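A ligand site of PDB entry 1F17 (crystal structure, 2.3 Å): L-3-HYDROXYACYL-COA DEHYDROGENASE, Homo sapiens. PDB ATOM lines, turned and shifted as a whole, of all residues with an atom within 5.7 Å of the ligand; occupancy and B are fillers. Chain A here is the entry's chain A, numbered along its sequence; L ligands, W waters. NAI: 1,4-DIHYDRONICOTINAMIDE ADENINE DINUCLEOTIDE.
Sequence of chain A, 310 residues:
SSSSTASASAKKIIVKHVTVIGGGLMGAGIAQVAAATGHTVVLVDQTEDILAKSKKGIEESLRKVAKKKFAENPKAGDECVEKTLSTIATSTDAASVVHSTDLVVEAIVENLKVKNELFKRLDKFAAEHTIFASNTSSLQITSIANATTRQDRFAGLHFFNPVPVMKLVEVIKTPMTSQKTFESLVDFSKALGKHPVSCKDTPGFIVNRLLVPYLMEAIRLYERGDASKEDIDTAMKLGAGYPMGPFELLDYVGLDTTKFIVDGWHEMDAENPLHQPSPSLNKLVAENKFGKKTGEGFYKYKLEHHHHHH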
ATOM      1  N   ILE A  21     -27.380   1.383 -15.378  1.00  0.00           N
ATOM      2  CA  ILE A  21     -27.654   0.309 -16.316  1.00  0.00           C
ATOM      3  C   ILE A  21     -26.940  -0.969 -15.931  1.00  0.00           C
ATOM      4  O   ILE A  21     -25.711  -1.049 -15.974  1.00  0.00           O
ATOM      5  CB  ILE A  21     -27.272   0.724 -17.761  1.00  0.00           C
ATOM      6  CG1 ILE A  21     -28.018   2.010 -18.127  1.00  0.00           C
ATOM      7  CG2 ILE A  21     -27.647  -0.370 -18.734  1.00  0.00           C
ATOM      8  CD1 ILE A  21     -27.700   2.547 -19.523  1.00  0.00           C
ATOM      9  N   GLY A  22     -27.721  -1.960 -15.551  1.00  0.00           N
ATOM     10  CA  GLY A  22     -27.185  -3.245 -15.138  1.00  0.00           C
ATOM     11  C   GLY A  22     -27.612  -3.474 -13.704  1.00  0.00           C
ATOM     12  O   GLY A  22     -27.141  -2.790 -12.796  1.00  0.00           O
ATOM     13  N   GLY A  23     -28.525  -4.429 -13.483  1.00  0.00           N
ATOM     14  CA  GLY A  23     -29.003  -4.691 -12.135  1.00  0.00           C
ATOM     15  C   GLY A  23     -28.352  -5.894 -11.475  1.00  0.00           C
ATOM     16  O   GLY A  23     -28.967  -6.564 -10.642  1.00  0.00           O
ATOM     17  N   GLY A  24     -27.099  -6.154 -11.837  1.00  0.00           N
ATOM     18  CA  GLY A  24     -26.375  -7.260 -11.251  1.00  0.00           C
ATOM     19  C   GLY A  24     -25.741  -6.852  -9.933  1.00  0.00           C
ATOM     20  O   GLY A  24     -26.110  -5.851  -9.325  1.00  0.00           O
ATOM     21  N   LEU A  25     -24.761  -7.634  -9.500  1.00  0.00           N
ATOM     22  CA  LEU A  25     -24.058  -7.381  -8.257  1.00  0.00           C
ATOM     23  C   LEU A  25     -23.671  -5.897  -8.072  1.00  0.00           C
ATOM     24  O   LEU A  25     -24.035  -5.275  -7.069  1.00  0.00           O
ATOM     25  CB  LEU A  25     -22.799  -8.252  -8.210  1.00  0.00           C
ATOM     26  CG  LEU A  25     -21.894  -8.169  -6.977  1.00  0.00           C
ATOM     27  CD1 LEU A  25     -22.636  -8.679  -5.759  1.00  0.00           C
ATOM     28  CD2 LEU A  25     -20.623  -8.986  -7.223  1.00  0.00           C
ATOM     29  N   MET A  26     -22.963  -5.333  -9.034  1.00  0.00           N
ATOM     30  CA  MET A  26     -22.502  -3.956  -8.959  1.00  0.00           C
ATOM     31  C   MET A  26     -23.542  -2.859  -9.189  1.00  0.00           C
ATOM     32  O   MET A  26     -23.656  -1.928  -8.377  1.00  0.00           O
ATOM     33  CB  MET A  26     -21.332  -3.748  -9.928  1.00  0.00           C
ATOM     34  CG  MET A  26     -20.154  -4.656  -9.659  1.00  0.00           C
ATOM     35  SD  MET A  26     -19.476  -4.454  -7.983  1.00  0.00           S
ATOM     36  CE  MET A  26     -18.912  -2.748  -8.026  1.00  0.00           C
ATOM     37  N   GLY A  27     -24.292  -2.964 -10.281  1.00  0.00           N
ATOM     38  CA  GLY A  27     -25.297  -1.961 -10.580  1.00  0.00           C
ATOM     39  C   GLY A  27     -26.352  -1.815  -9.509  1.00  0.00           C
ATOM     40  O   GLY A  27     -26.778  -0.710  -9.186  1.00  0.00           O
ATOM     41  N   VAL A  44     -31.906  -0.080 -14.819  1.00  0.00           N
ATOM     42  CA  VAL A  44     -32.239  -0.684 -16.092  1.00  0.00           C
ATOM     43  C   VAL A  44     -31.641  -2.061 -16.295  1.00  0.00           C
ATOM     44  O   VAL A  44     -30.509  -2.317 -15.880  1.00  0.00           O
ATOM     45  CB  VAL A  44     -31.756   0.220 -17.262  1.00  0.00           C
ATOM     46  CG1 VAL A  44     -31.971  -0.450 -18.609  1.00  0.00           C
ATOM     47  CG2 VAL A  44     -32.458   1.560 -17.180  1.00  0.00           C
ATOM     48  N   ASP A  45     -32.405  -2.938 -16.942  1.00  0.00           N
ATOM     49  CA  ASP A  45     -31.933  -4.277 -17.266  1.00  0.00           C
ATOM     50  C   ASP A  45     -32.835  -4.884 -18.348  1.00  0.00           C
ATOM     51  O   ASP A  45     -33.888  -4.356 -18.661  1.00  0.00           O
ATOM     52  CB  ASP A  45     -31.872  -5.183 -16.027  1.00  0.00           C
ATOM     53  CG  ASP A  45     -30.690  -6.147 -16.084  1.00  0.00           C
ATOM     54  OD1 ASP A  45     -30.610  -6.969 -17.032  1.00  0.00           O
ATOM     55  OD2 ASP A  45     -29.821  -6.069 -15.197  1.00  0.00           O
ATOM     56  N   GLN A  46     -32.392  -6.001 -18.902  1.00  0.00           N
ATOM     57  CA  GLN A  46     -33.083  -6.641 -20.010  1.00  0.00           C
ATOM     58  C   GLN A  46     -34.561  -7.010 -19.852  1.00  0.00           C
ATOM     59  O   GLN A  46     -35.325  -6.805 -20.785  1.00  0.00           O
ATOM     60  CB  GLN A  46     -32.274  -7.847 -20.457  1.00  0.00           C
ATOM     61  CG  GLN A  46     -30.845  -7.474 -20.861  1.00  0.00           C
ATOM     62  CD  GLN A  46     -29.987  -8.675 -21.227  1.00  0.00           C
ATOM     63  OE1 GLN A  46     -30.248  -9.363 -22.211  1.00  0.00           O
ATOM     64  NE2 GLN A  46     -28.954  -8.933 -20.423  1.00  0.00           N
ATOM     65  N   ILE A  50     -35.704  -9.868 -14.269  1.00  0.00           N
ATOM     66  CA  ILE A  50     -34.359  -9.534 -13.817  1.00  0.00           C
ATOM     67  C   ILE A  50     -34.464  -8.308 -12.915  1.00  0.00           C
ATOM     68  O   ILE A  50     -33.880  -8.271 -11.835  1.00  0.00           O
ATOM     69  CB  ILE A  50     -33.436  -9.227 -15.004  1.00  0.00           C
ATOM     70  CG1 ILE A  50     -33.338 -10.452 -15.913  1.00  0.00           C
ATOM     71  CG2 ILE A  50     -32.054  -8.777 -14.489  1.00  0.00           C
ATOM     72  CD1 ILE A  50     -32.485 -10.244 -17.155  1.00  0.00           C
ATOM     73  N   SER A  54     -33.719  -7.877  -9.044  1.00  0.00           N
ATOM     74  CA  SER A  54     -32.657  -6.958  -8.615  1.00  0.00           C
ATOM     75  C   SER A  54     -33.158  -6.047  -7.523  1.00  0.00           C
ATOM     76  O   SER A  54     -32.540  -5.909  -6.466  1.00  0.00           O
ATOM     77  CB  SER A  54     -32.166  -6.090  -9.787  1.00  0.00           C
ATOM     78  OG  SER A  54     -31.533  -6.871 -10.778  1.00  0.00           O
ATOM     79  N   GLU A 106     -23.063   2.830 -16.178  1.00  0.00           N
ATOM     80  CA  GLU A 106     -23.214   1.513 -16.758  1.00  0.00           C
ATOM     81  C   GLU A 106     -22.445   0.418 -16.031  1.00  0.00           C
ATOM     82  O   GLU A 106     -21.261   0.575 -15.734  1.00  0.00           O
ATOM     83  CB  GLU A 106     -22.805   1.558 -18.247  1.00  0.00           C
ATOM     84  CG  GLU A 106     -22.620   0.200 -18.935  1.00  0.00           C
ATOM     85  CD  GLU A 106     -21.235  -0.383 -18.686  1.00  0.00           C
ATOM     86  OE1 GLU A 106     -20.254   0.360 -18.882  1.00  0.00           O
ATOM     87  OE2 GLU A 106     -21.134  -1.578 -18.327  1.00  0.00           O
ATOM     88  N   ALA A 107     -23.116  -0.692 -15.755  1.00  0.00           N
ATOM     89  CA  ALA A 107     -22.497  -1.815 -15.074  1.00  0.00           C
ATOM     90  C   ALA A 107     -23.086  -3.105 -15.622  1.00  0.00           C
ATOM     91  O   ALA A 107     -23.684  -3.885 -14.889  1.00  0.00           O
ATOM     92  CB  ALA A 107     -22.738  -1.731 -13.559  1.00  0.00           C
ATOM     93  N   ILE A 108     -22.917  -3.311 -16.930  1.00  0.00           N
ATOM     94  CA  ILE A 108     -23.440  -4.506 -17.589  1.00  0.00           C
ATOM     95  C   ILE A 108     -22.301  -5.449 -17.908  1.00  0.00           C
ATOM     96  O   ILE A 108     -21.165  -5.200 -17.515  1.00  0.00           O
ATOM     97  CB  ILE A 108     -24.173  -4.143 -18.906  1.00  0.00           C
ATOM     98  CG1 ILE A 108     -23.181  -3.578 -19.929  1.00  0.00           C
ATOM     99  CG2 ILE A 108     -25.263  -3.128 -18.617  1.00  0.00           C
ATOM    100  CD1 ILE A 108     -23.819  -3.173 -21.257  1.00  0.00           C
ATOM    101  N   VAL A 109     -22.602  -6.537 -18.628  1.00  0.00           N
ATOM    102  CA  VAL A 109     -21.604  -7.531 -18.993  1.00  0.00           C
ATOM    103  C   VAL A 109     -20.298  -6.880 -19.437  1.00  0.00           C
ATOM    104  O   VAL A 109     -20.289  -5.900 -20.178  1.00  0.00           O
ATOM    105  CB  VAL A 109     -22.108  -8.457 -20.139  1.00  0.00           C
ATOM    106  CG1 VAL A 109     -22.403  -7.638 -21.401  1.00  0.00           C
ATOM    107  CG2 VAL A 109     -21.081  -9.530 -20.424  1.00  0.00           C
ATOM    108  N   GLU A 110     -19.184  -7.444 -18.967  1.00  0.00           N
ATOM    109  CA  GLU A 110     -17.857  -6.930 -19.269  1.00  0.00           C
ATOM    110  C   GLU A 110     -17.430  -7.276 -20.701  1.00  0.00           C
ATOM    111  O   GLU A 110     -16.524  -8.087 -20.920  1.00  0.00           O
ATOM    112  CB  GLU A 110     -16.852  -7.487 -18.258  1.00  0.00           C
ATOM    113  CG  GLU A 110     -15.438  -6.924 -18.364  1.00  0.00           C
ATOM    114  CD  GLU A 110     -15.280  -5.535 -17.744  1.00  0.00           C
ATOM    115  OE1 GLU A 110     -16.058  -4.616 -18.084  1.00  0.00           O
ATOM    116  OE2 GLU A 110     -14.370  -5.353 -16.912  1.00  0.00           O
ATOM    117  N   VAL A 114     -20.591  -4.935 -26.592  1.00  0.00           N
ATOM    118  CA  VAL A 114     -21.912  -4.732 -26.026  1.00  0.00           C
ATOM    119  C   VAL A 114     -21.999  -3.347 -25.397  1.00  0.00           C
ATOM    120  O   VAL A 114     -22.985  -2.639 -25.562  1.00  0.00           O
ATOM    121  CB  VAL A 114     -22.228  -5.810 -24.973  1.00  0.00           C
ATOM    122  CG1 VAL A 114     -23.637  -5.597 -24.418  1.00  0.00           C
ATOM    123  CG2 VAL A 114     -22.141  -7.186 -25.613  1.00  0.00           C
ATOM    124  N   LYS A 115     -20.947  -2.949 -24.677  1.00  0.00           N
ATOM    125  CA  LYS A 115     -20.910  -1.644 -24.033  1.00  0.00           C
ATOM    126  C   LYS A 115     -20.902  -0.509 -25.059  1.00  0.00           C
ATOM    127  O   LYS A 115     -21.644   0.469 -24.927  1.00  0.00           O
ATOM    128  CB  LYS A 115     -19.682  -1.513 -23.125  1.00  0.00           C
ATOM    129  CG  LYS A 115     -19.771  -2.248 -21.771  1.00  0.00           C
ATOM    130  CD  LYS A 115     -18.384  -2.260 -21.091  1.00  0.00           C
ATOM    131  CE  LYS A 115     -18.437  -2.512 -19.571  1.00  0.00           C
ATOM    132  NZ  LYS A 115     -19.218  -3.683 -19.136  1.00  0.00           N
ATOM    133  N   LEU A 118     -24.264  -0.117 -26.608  1.00  0.00           N
ATOM    134  CA  LEU A 118     -25.135   0.527 -25.636  1.00  0.00           C
ATOM    135  C   LEU A 118     -24.966   2.043 -25.669  1.00  0.00           C
ATOM    136  O   LEU A 118     -25.915   2.788 -25.917  1.00  0.00           O
ATOM    137  CB  LEU A 118     -24.812   0.009 -24.243  1.00  0.00           C
ATOM    138  CG  LEU A 118     -25.610   0.666 -23.112  1.00  0.00           C
ATOM    139  CD1 LEU A 118     -27.054   0.208 -23.219  1.00  0.00           C
ATOM    140  CD2 LEU A 118     -25.015   0.277 -21.766  1.00  0.00           C
ATOM    141  N   ASN A 135     -18.483   1.483 -15.234  1.00  0.00           N
ATOM    142  CA  ASN A 135     -17.937   0.872 -14.009  1.00  0.00           C
ATOM    143  C   ASN A 135     -17.035  -0.306 -14.369  1.00  0.00           C
ATOM    144  O   ASN A 135     -16.717  -1.133 -13.524  1.00  0.00           O
ATOM    145  CB  ASN A 135     -19.106   0.419 -13.128  1.00  0.00           C
ATOM    146  CG  ASN A 135     -18.650  -0.278 -11.836  1.00  0.00           C
ATOM    147  OD1 ASN A 135     -17.948   0.308 -11.017  1.00  0.00           O
ATOM    148  ND2 ASN A 135     -19.084  -1.513 -11.663  1.00  0.00           N
ATOM    149  N   THR A 136     -16.608  -0.380 -15.637  1.00  0.00           N
ATOM    150  CA  THR A 136     -15.774  -1.496 -16.086  1.00  0.00           C
ATOM    151  C   THR A 136     -14.459  -1.638 -15.341  1.00  0.00           C
ATOM    152  O   THR A 136     -13.854  -0.641 -14.920  1.00  0.00           O
ATOM    153  CB  THR A 136     -15.452  -1.394 -17.604  1.00  0.00           C
ATOM    154  OG1 THR A 136     -14.651  -2.521 -17.996  1.00  0.00           O
ATOM    155  CG2 THR A 136     -14.689  -0.110 -17.911  1.00  0.00           C
ATOM    156  N   SER A 137     -13.998  -2.872 -15.181  1.00  0.00           N
ATOM    157  CA  SER A 137     -12.743  -3.137 -14.492  1.00  0.00           C
ATOM    158  C   SER A 137     -11.587  -3.435 -15.431  1.00  0.00           C
ATOM    159  O   SER A 137     -10.434  -3.205 -15.072  1.00  0.00           O
ATOM    160  CB  SER A 137     -12.879  -4.334 -13.542  1.00  0.00           C
ATOM    161  OG  SER A 137     -13.704  -4.022 -12.440  1.00  0.00           O
ATOM    162  N   SER A 138     -11.870  -3.917 -16.638  1.00  0.00           N
ATOM    163  CA  SER A 138     -10.789  -4.262 -17.544  1.00  0.00           C
ATOM    164  C   SER A 138     -10.728  -3.566 -18.908  1.00  0.00           C
ATOM    165  O   SER A 138      -9.710  -3.606 -19.582  1.00  0.00           O
ATOM    166  CB  SER A 138     -10.771  -5.779 -17.745  1.00  0.00           C
ATOM    167  OG  SER A 138     -12.030  -6.248 -18.213  1.00  0.00           O
ATOM    168  N   HIS A 158     -15.489   3.799 -11.134  1.00  0.00           N
ATOM    169  CA  HIS A 158     -15.265   2.427 -10.683  1.00  0.00           C
ATOM    170  C   HIS A 158     -15.536   2.162  -9.209  1.00  0.00           C
ATOM    171  O   HIS A 158     -14.858   2.713  -8.334  1.00  0.00           O
ATOM    172  CB  HIS A 158     -13.819   2.059 -11.030  1.00  0.00           C
ATOM    173  CG  HIS A 158     -13.512   0.600 -10.945  1.00  0.00           C
ATOM    174  ND1 HIS A 158     -12.371   0.124 -10.353  1.00  0.00           N
ATOM    175  CD2 HIS A 158     -14.172  -0.477 -11.417  1.00  0.00           C
ATOM    176  CE1 HIS A 158     -12.340  -1.199 -10.464  1.00  0.00           C
ATOM    177  NE2 HIS A 158     -13.426  -1.583 -11.106  1.00  0.00           N
ATOM    178  N   PHE A 159     -16.514   1.297  -8.920  1.00  0.00           N
ATOM    179  CA  PHE A 159     -16.850   0.979  -7.537  1.00  0.00           C
ATOM    180  C   PHE A 159     -16.279  -0.354  -7.057  1.00  0.00           C
ATOM    181  O   PHE A 159     -15.589  -1.047  -7.800  1.00  0.00           O
ATOM    182  CB  PHE A 159     -18.366   0.940  -7.348  1.00  0.00           C
ATOM    183  CG  PHE A 159     -19.035   2.243  -7.644  1.00  0.00           C
ATOM    184  CD1 PHE A 159     -19.266   2.647  -8.954  1.00  0.00           C
ATOM    185  CD2 PHE A 159     -19.422   3.086  -6.607  1.00  0.00           C
ATOM    186  CE1 PHE A 159     -19.874   3.869  -9.229  1.00  0.00           C
ATOM    187  CE2 PHE A 159     -20.021   4.312  -6.862  1.00  0.00           C
ATOM    188  CZ  PHE A 159     -20.250   4.703  -8.192  1.00  0.00           C
ATOM    189  N   PHE A 160     -16.567  -0.687  -5.809  1.00  0.00           N
ATOM    190  CA  PHE A 160     -16.072  -1.919  -5.232  1.00  0.00           C
ATOM    191  C   PHE A 160     -17.171  -2.650  -4.471  1.00  0.00           C
ATOM    192  O   PHE A 160     -17.960  -2.044  -3.753  1.00  0.00           O
ATOM    193  CB  PHE A 160     -14.864  -1.663  -4.331  1.00  0.00           C
ATOM    194  CG  PHE A 160     -13.699  -1.051  -5.058  1.00  0.00           C
ATOM    195  CD1 PHE A 160     -13.747   0.260  -5.510  1.00  0.00           C
ATOM    196  CD2 PHE A 160     -12.576  -1.811  -5.346  1.00  0.00           C
ATOM    197  CE1 PHE A 160     -12.707   0.800  -6.247  1.00  0.00           C
ATOM    198  CE2 PHE A 160     -11.531  -1.277  -6.088  1.00  0.00           C
ATOM    199  CZ  PHE A 160     -11.603   0.037  -6.545  1.00  0.00           C
ATOM    200  N   ASN A 161     -17.208  -3.956  -4.652  1.00  0.00           N
ATOM    201  CA  ASN A 161     -18.202  -4.803  -4.020  1.00  0.00           C
ATOM    202  C   ASN A 161     -17.832  -5.181  -2.583  1.00  0.00           C
ATOM    203  O   ASN A 161     -16.671  -5.487  -2.293  1.00  0.00           O
ATOM    204  CB  ASN A 161     -18.381  -6.075  -4.843  1.00  0.00           C
ATOM    205  CG  ASN A 161     -19.265  -7.098  -4.162  1.00  0.00           C
ATOM    206  OD1 ASN A 161     -20.439  -6.857  -3.923  1.00  0.00           O
ATOM    207  ND2 ASN A 161     -18.674  -8.253  -3.841  1.00  0.00           N
ATOM    208  N   VAL A 253     -13.536 -12.692  -4.346  1.00  0.00           N
ATOM    209  CA  VAL A 253     -13.780 -11.814  -5.501  1.00  0.00           C
ATOM    210  C   VAL A 253     -14.162 -12.586  -6.769  1.00  0.00           C
ATOM    211  O   VAL A 253     -14.728 -12.002  -7.688  1.00  0.00           O
ATOM    212  CB  VAL A 253     -12.557 -10.900  -5.818  1.00  0.00           C
ATOM    213  CG1 VAL A 253     -12.224 -10.036  -4.608  1.00  0.00           C
ATOM    214  CG2 VAL A 253     -11.355 -11.719  -6.251  1.00  0.00           C
ATOM    215  N   THR A 257     -13.555 -14.046 -12.391  1.00  0.00           N
ATOM    216  CA  THR A 257     -13.440 -12.605 -12.462  1.00  0.00           C
ATOM    217  C   THR A 257     -11.952 -12.221 -12.527  1.00  0.00           C
ATOM    218  O   THR A 257     -11.556 -11.362 -13.316  1.00  0.00           O
ATOM    219  CB  THR A 257     -14.071 -11.973 -11.229  1.00  0.00           C
ATOM    220  OG1 THR A 257     -15.336 -12.591 -10.998  1.00  0.00           O
ATOM    221  CG2 THR A 257     -14.276 -10.480 -11.430  1.00  0.00           C
HETATM  222  PA  NAI L   1     -23.520  -9.082 -13.240  1.00  0.00           P
HETATM  223  O1A NAI L   1     -23.568 -10.121 -14.288  1.00  0.00           O
HETATM  224  O2A NAI L   1     -23.847  -9.590 -11.884  1.00  0.00           O
HETATM  225  O5B NAI L   1     -24.515  -7.884 -13.656  1.00  0.00           O
HETATM  226  C5B NAI L   1     -24.612  -7.395 -15.018  1.00  0.00           C
HETATM  227  C4B NAI L   1     -26.062  -7.113 -15.376  1.00  0.00           C
HETATM  228  O4B NAI L   1     -26.005  -6.571 -16.718  1.00  0.00           O
HETATM  229  C3B NAI L   1     -26.981  -8.340 -15.510  1.00  0.00           C
HETATM  230  O3B NAI L   1     -28.121  -8.207 -14.641  1.00  0.00           O
HETATM  231  C2B NAI L   1     -27.337  -8.386 -17.006  1.00  0.00           C
HETATM  232  O2B NAI L   1     -28.661  -8.902 -17.298  1.00  0.00           O
HETATM  233  C1B NAI L   1     -27.159  -6.935 -17.401  1.00  0.00           C
HETATM  234  N9A NAI L   1     -26.974  -6.659 -18.832  1.00  0.00           N
HETATM  235  C8A NAI L   1     -26.216  -7.303 -19.768  1.00  0.00           C
HETATM  236  N7A NAI L   1     -26.308  -6.789 -21.001  1.00  0.00           N
HETATM  237  C5A NAI L   1     -27.195  -5.740 -20.856  1.00  0.00           C
HETATM  238  C6A NAI L   1     -27.750  -4.770 -21.720  1.00  0.00           C
HETATM  239  N6A NAI L   1     -27.511  -4.662 -23.017  1.00  0.00           N
HETATM  240  N1A NAI L   1     -28.606  -3.829 -21.237  1.00  0.00           N
HETATM  241  C2A NAI L   1     -28.908  -3.872 -19.891  1.00  0.00           C
HETATM  242  N3A NAI L   1     -28.463  -4.726 -19.006  1.00  0.00           N
HETATM  243  C4A NAI L   1     -27.604  -5.633 -19.526  1.00  0.00           C
HETATM  244  O3  NAI L   1     -22.103  -8.454 -13.248  1.00  0.00           O
HETATM  245  PN  NAI L   1     -21.298  -7.354 -12.334  1.00  0.00           P
HETATM  246  O1N NAI L   1     -20.381  -8.174 -11.527  1.00  0.00           O
HETATM  247  O2N NAI L   1     -22.339  -6.627 -11.571  1.00  0.00           O
HETATM  248  O5D NAI L   1     -20.440  -6.552 -13.410  1.00  0.00           O
HETATM  249  C5D NAI L   1     -20.749  -5.179 -13.653  1.00  0.00           C
HETATM  250  C4D NAI L   1     -19.699  -4.515 -14.510  1.00  0.00           C
HETATM  251  O4D NAI L   1     -18.918  -3.938 -13.432  1.00  0.00           O
HETATM  252  C3D NAI L   1     -18.672  -5.272 -15.351  1.00  0.00           C
HETATM  253  O3D NAI L   1     -18.221  -4.429 -16.422  1.00  0.00           O
HETATM  254  C2D NAI L   1     -17.518  -5.532 -14.369  1.00  0.00           C
HETATM  255  O2D NAI L   1     -16.240  -5.707 -15.000  1.00  0.00           O
HETATM  256  C1D NAI L   1     -17.576  -4.335 -13.448  1.00  0.00           C
HETATM  257  N1N NAI L   1     -17.161  -4.567 -12.062  1.00  0.00           N
HETATM  258  C2N NAI L   1     -17.393  -5.762 -11.356  1.00  0.00           C
HETATM  259  C3N NAI L   1     -16.866  -5.977  -9.974  1.00  0.00           C
HETATM  260  C7N NAI L   1     -17.193  -7.240  -9.279  1.00  0.00           C
HETATM  261  O7N NAI L   1     -16.728  -7.407  -8.135  1.00  0.00           O
HETATM  262  N7N NAI L   1     -18.003  -8.208  -9.750  1.00  0.00           N
HETATM  263  C4N NAI L   1     -16.150  -4.813  -9.339  1.00  0.00           C
HETATM  264  C5N NAI L   1     -16.011  -3.583 -10.172  1.00  0.00           C
HETATM  265  C6N NAI L   1     -16.473  -3.474 -11.416  1.00  0.00           C
HETATM  266  O   HOH W   1     -12.792  -4.799  -9.343  1.00  0.00           O
HETATM  267  O   HOH W   2     -28.709  -9.750 -12.276  1.00  0.00           O
HETATM  268  O   HOH W   3     -31.650  -2.870 -21.087  1.00  0.00           O
HETATM  269  O   HOH W   4     -24.690 -10.222 -18.280  1.00  0.00           O
HETATM  270  O   HOH W   5     -24.382  -4.869 -12.283  1.00  0.00           O
HETATM  271  O   HOH W   6     -19.072  -1.802 -15.985  1.00  0.00           O
HETATM  272  O   HOH W   7     -15.136  -5.287  -6.126  1.00  0.00           O
HETATM  273  O   HOH W   8     -13.877  -6.829 -11.351  1.00  0.00           O
HETATM  274  O   HOH W   9     -15.465  -7.771 -13.516  1.00  0.00           O
HETATM  275  O   HOH W  10     -22.336 -10.367 -16.563  1.00  0.00           O
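An oxygen (O2D) of the ligand sits at hydrogen-bond distance from the side-chain carboxylate (OE2) of Glu 110 (2.7 Å). O2B of the ligand is in hydrogen-bond range of OD1 of Asp 45 (2.8 Å). N of Met 26 lies within hydrogen-bond range of O2N of the ligand (2.9 Å). The side-chain amino group (NZ) of Lys 115 is in hydrogen-bond range of an oxygen (O3D) of the ligand (3.0 Å). ND2 of Asn 135 sits at hydrogen-bond distance from O4D of the ligand (3.0 Å). O2B of the ligand lies within hydrogen-bond range of NE2 of Gln 46, at 3.1 Å. N of Leu 25 lies within hydrogen-bond range of O2A of the ligand (3.2 Å). The backbone carbonyl oxygen (O) of Ile 108 is in hydrogen-bond range of an oxygen (O3D) of the ligand (3.2 Å).
The side-chain carboxylate (OD2) of Asp 45 is in hydrogen-bond range of the backbone NH (N) of Gly 23, at 2.7 Å. O of Val 109 is in hydrogen-bond range of NZ of Lys 115 (2.7 Å). NZ of Lys 115 is in salt-bridge range of OE2 of Glu 106. OG of Ser 137 is in hydrogen-bond range of NE2 of His 158, 2.8 Å away. N of Phe 159 lies within hydrogen-bond range of OD1 of Asn 135, at 2.7 Å. The backbone carbonyl oxygen (O) of Glu 106 lies within hydrogen-bond range of the backbone NH (N) of Asn 135 (3.0 Å). N of Gly 22 is in hydrogen-bond range of O of Val 44. The side-chain hydroxyl (OG) of Ser 54 is in hydrogen-bond range of the backbone carbonyl oxygen (O) of Ile 50 (2.9 Å).
CG2 of Ile 21 touches C2A of the ligand, 3.9 Å away. CA of Gly 22 touches O4B of the ligand, 3.9 Å away. Gly 23 touches the ligand (C to O3B, 3.9 Å). CA of Gly 24 touches O5B of the ligand (3.1 Å). Ile 50 touches the ligand. Ala 107 touches the ligand. N of Val 109 touches C8A of the ligand (3.9 Å). Thr 136 touches the ligand. Ser 137 touches the ligand (OG to C6N, 3.0 Å). His 158 touches the ligand. Phe 159 touches the ligand (O to C5N, 3.5 Å). CB of Asn 161 touches O7N of the ligand, 3.9 Å away. 20 residues have an atom within 4 Å of the ligand: Ile 21, Gly 22, Gly 23, Gly 24, Leu 25, Met 26, Asp 45, Gln 46, Ile 50, Ala 107, Ile 108, Val 109, Glu 110, Lys 115, Asn 135, Thr 136, Ser 137, His 158, Phe 159 and Asn 161. The nearest printed residue that does not touch the ligand is Val 114 (4.2 Å).
Water W5 lies within hydrogen-bond range of the backbone NH of Gly 27 (2.8 Å), an oxygen (O2N) of the ligand (2.8 Å), the backbone carbonyl oxygen of Ala 107 (2.9 Å), the backbone NH of Gly 24 (3.0 Å) and the backbone carbonyl oxygen of Gly 22 (3.5 Å). Water W6 lies within hydrogen-bond range of an oxygen (O3D) of the ligand (2.8 Å), the backbone NH (N) of Thr 136 (2.9 Å), the side-chain carboxylate (OE2) of Glu 106 (3.1 Å) and the backbone NH (N) of Asn 135 (3.4 Å). Water W7 lies within hydrogen-bond range of N of Asn 161 (2.9 Å) and O7N of the ligand (3.3 Å).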
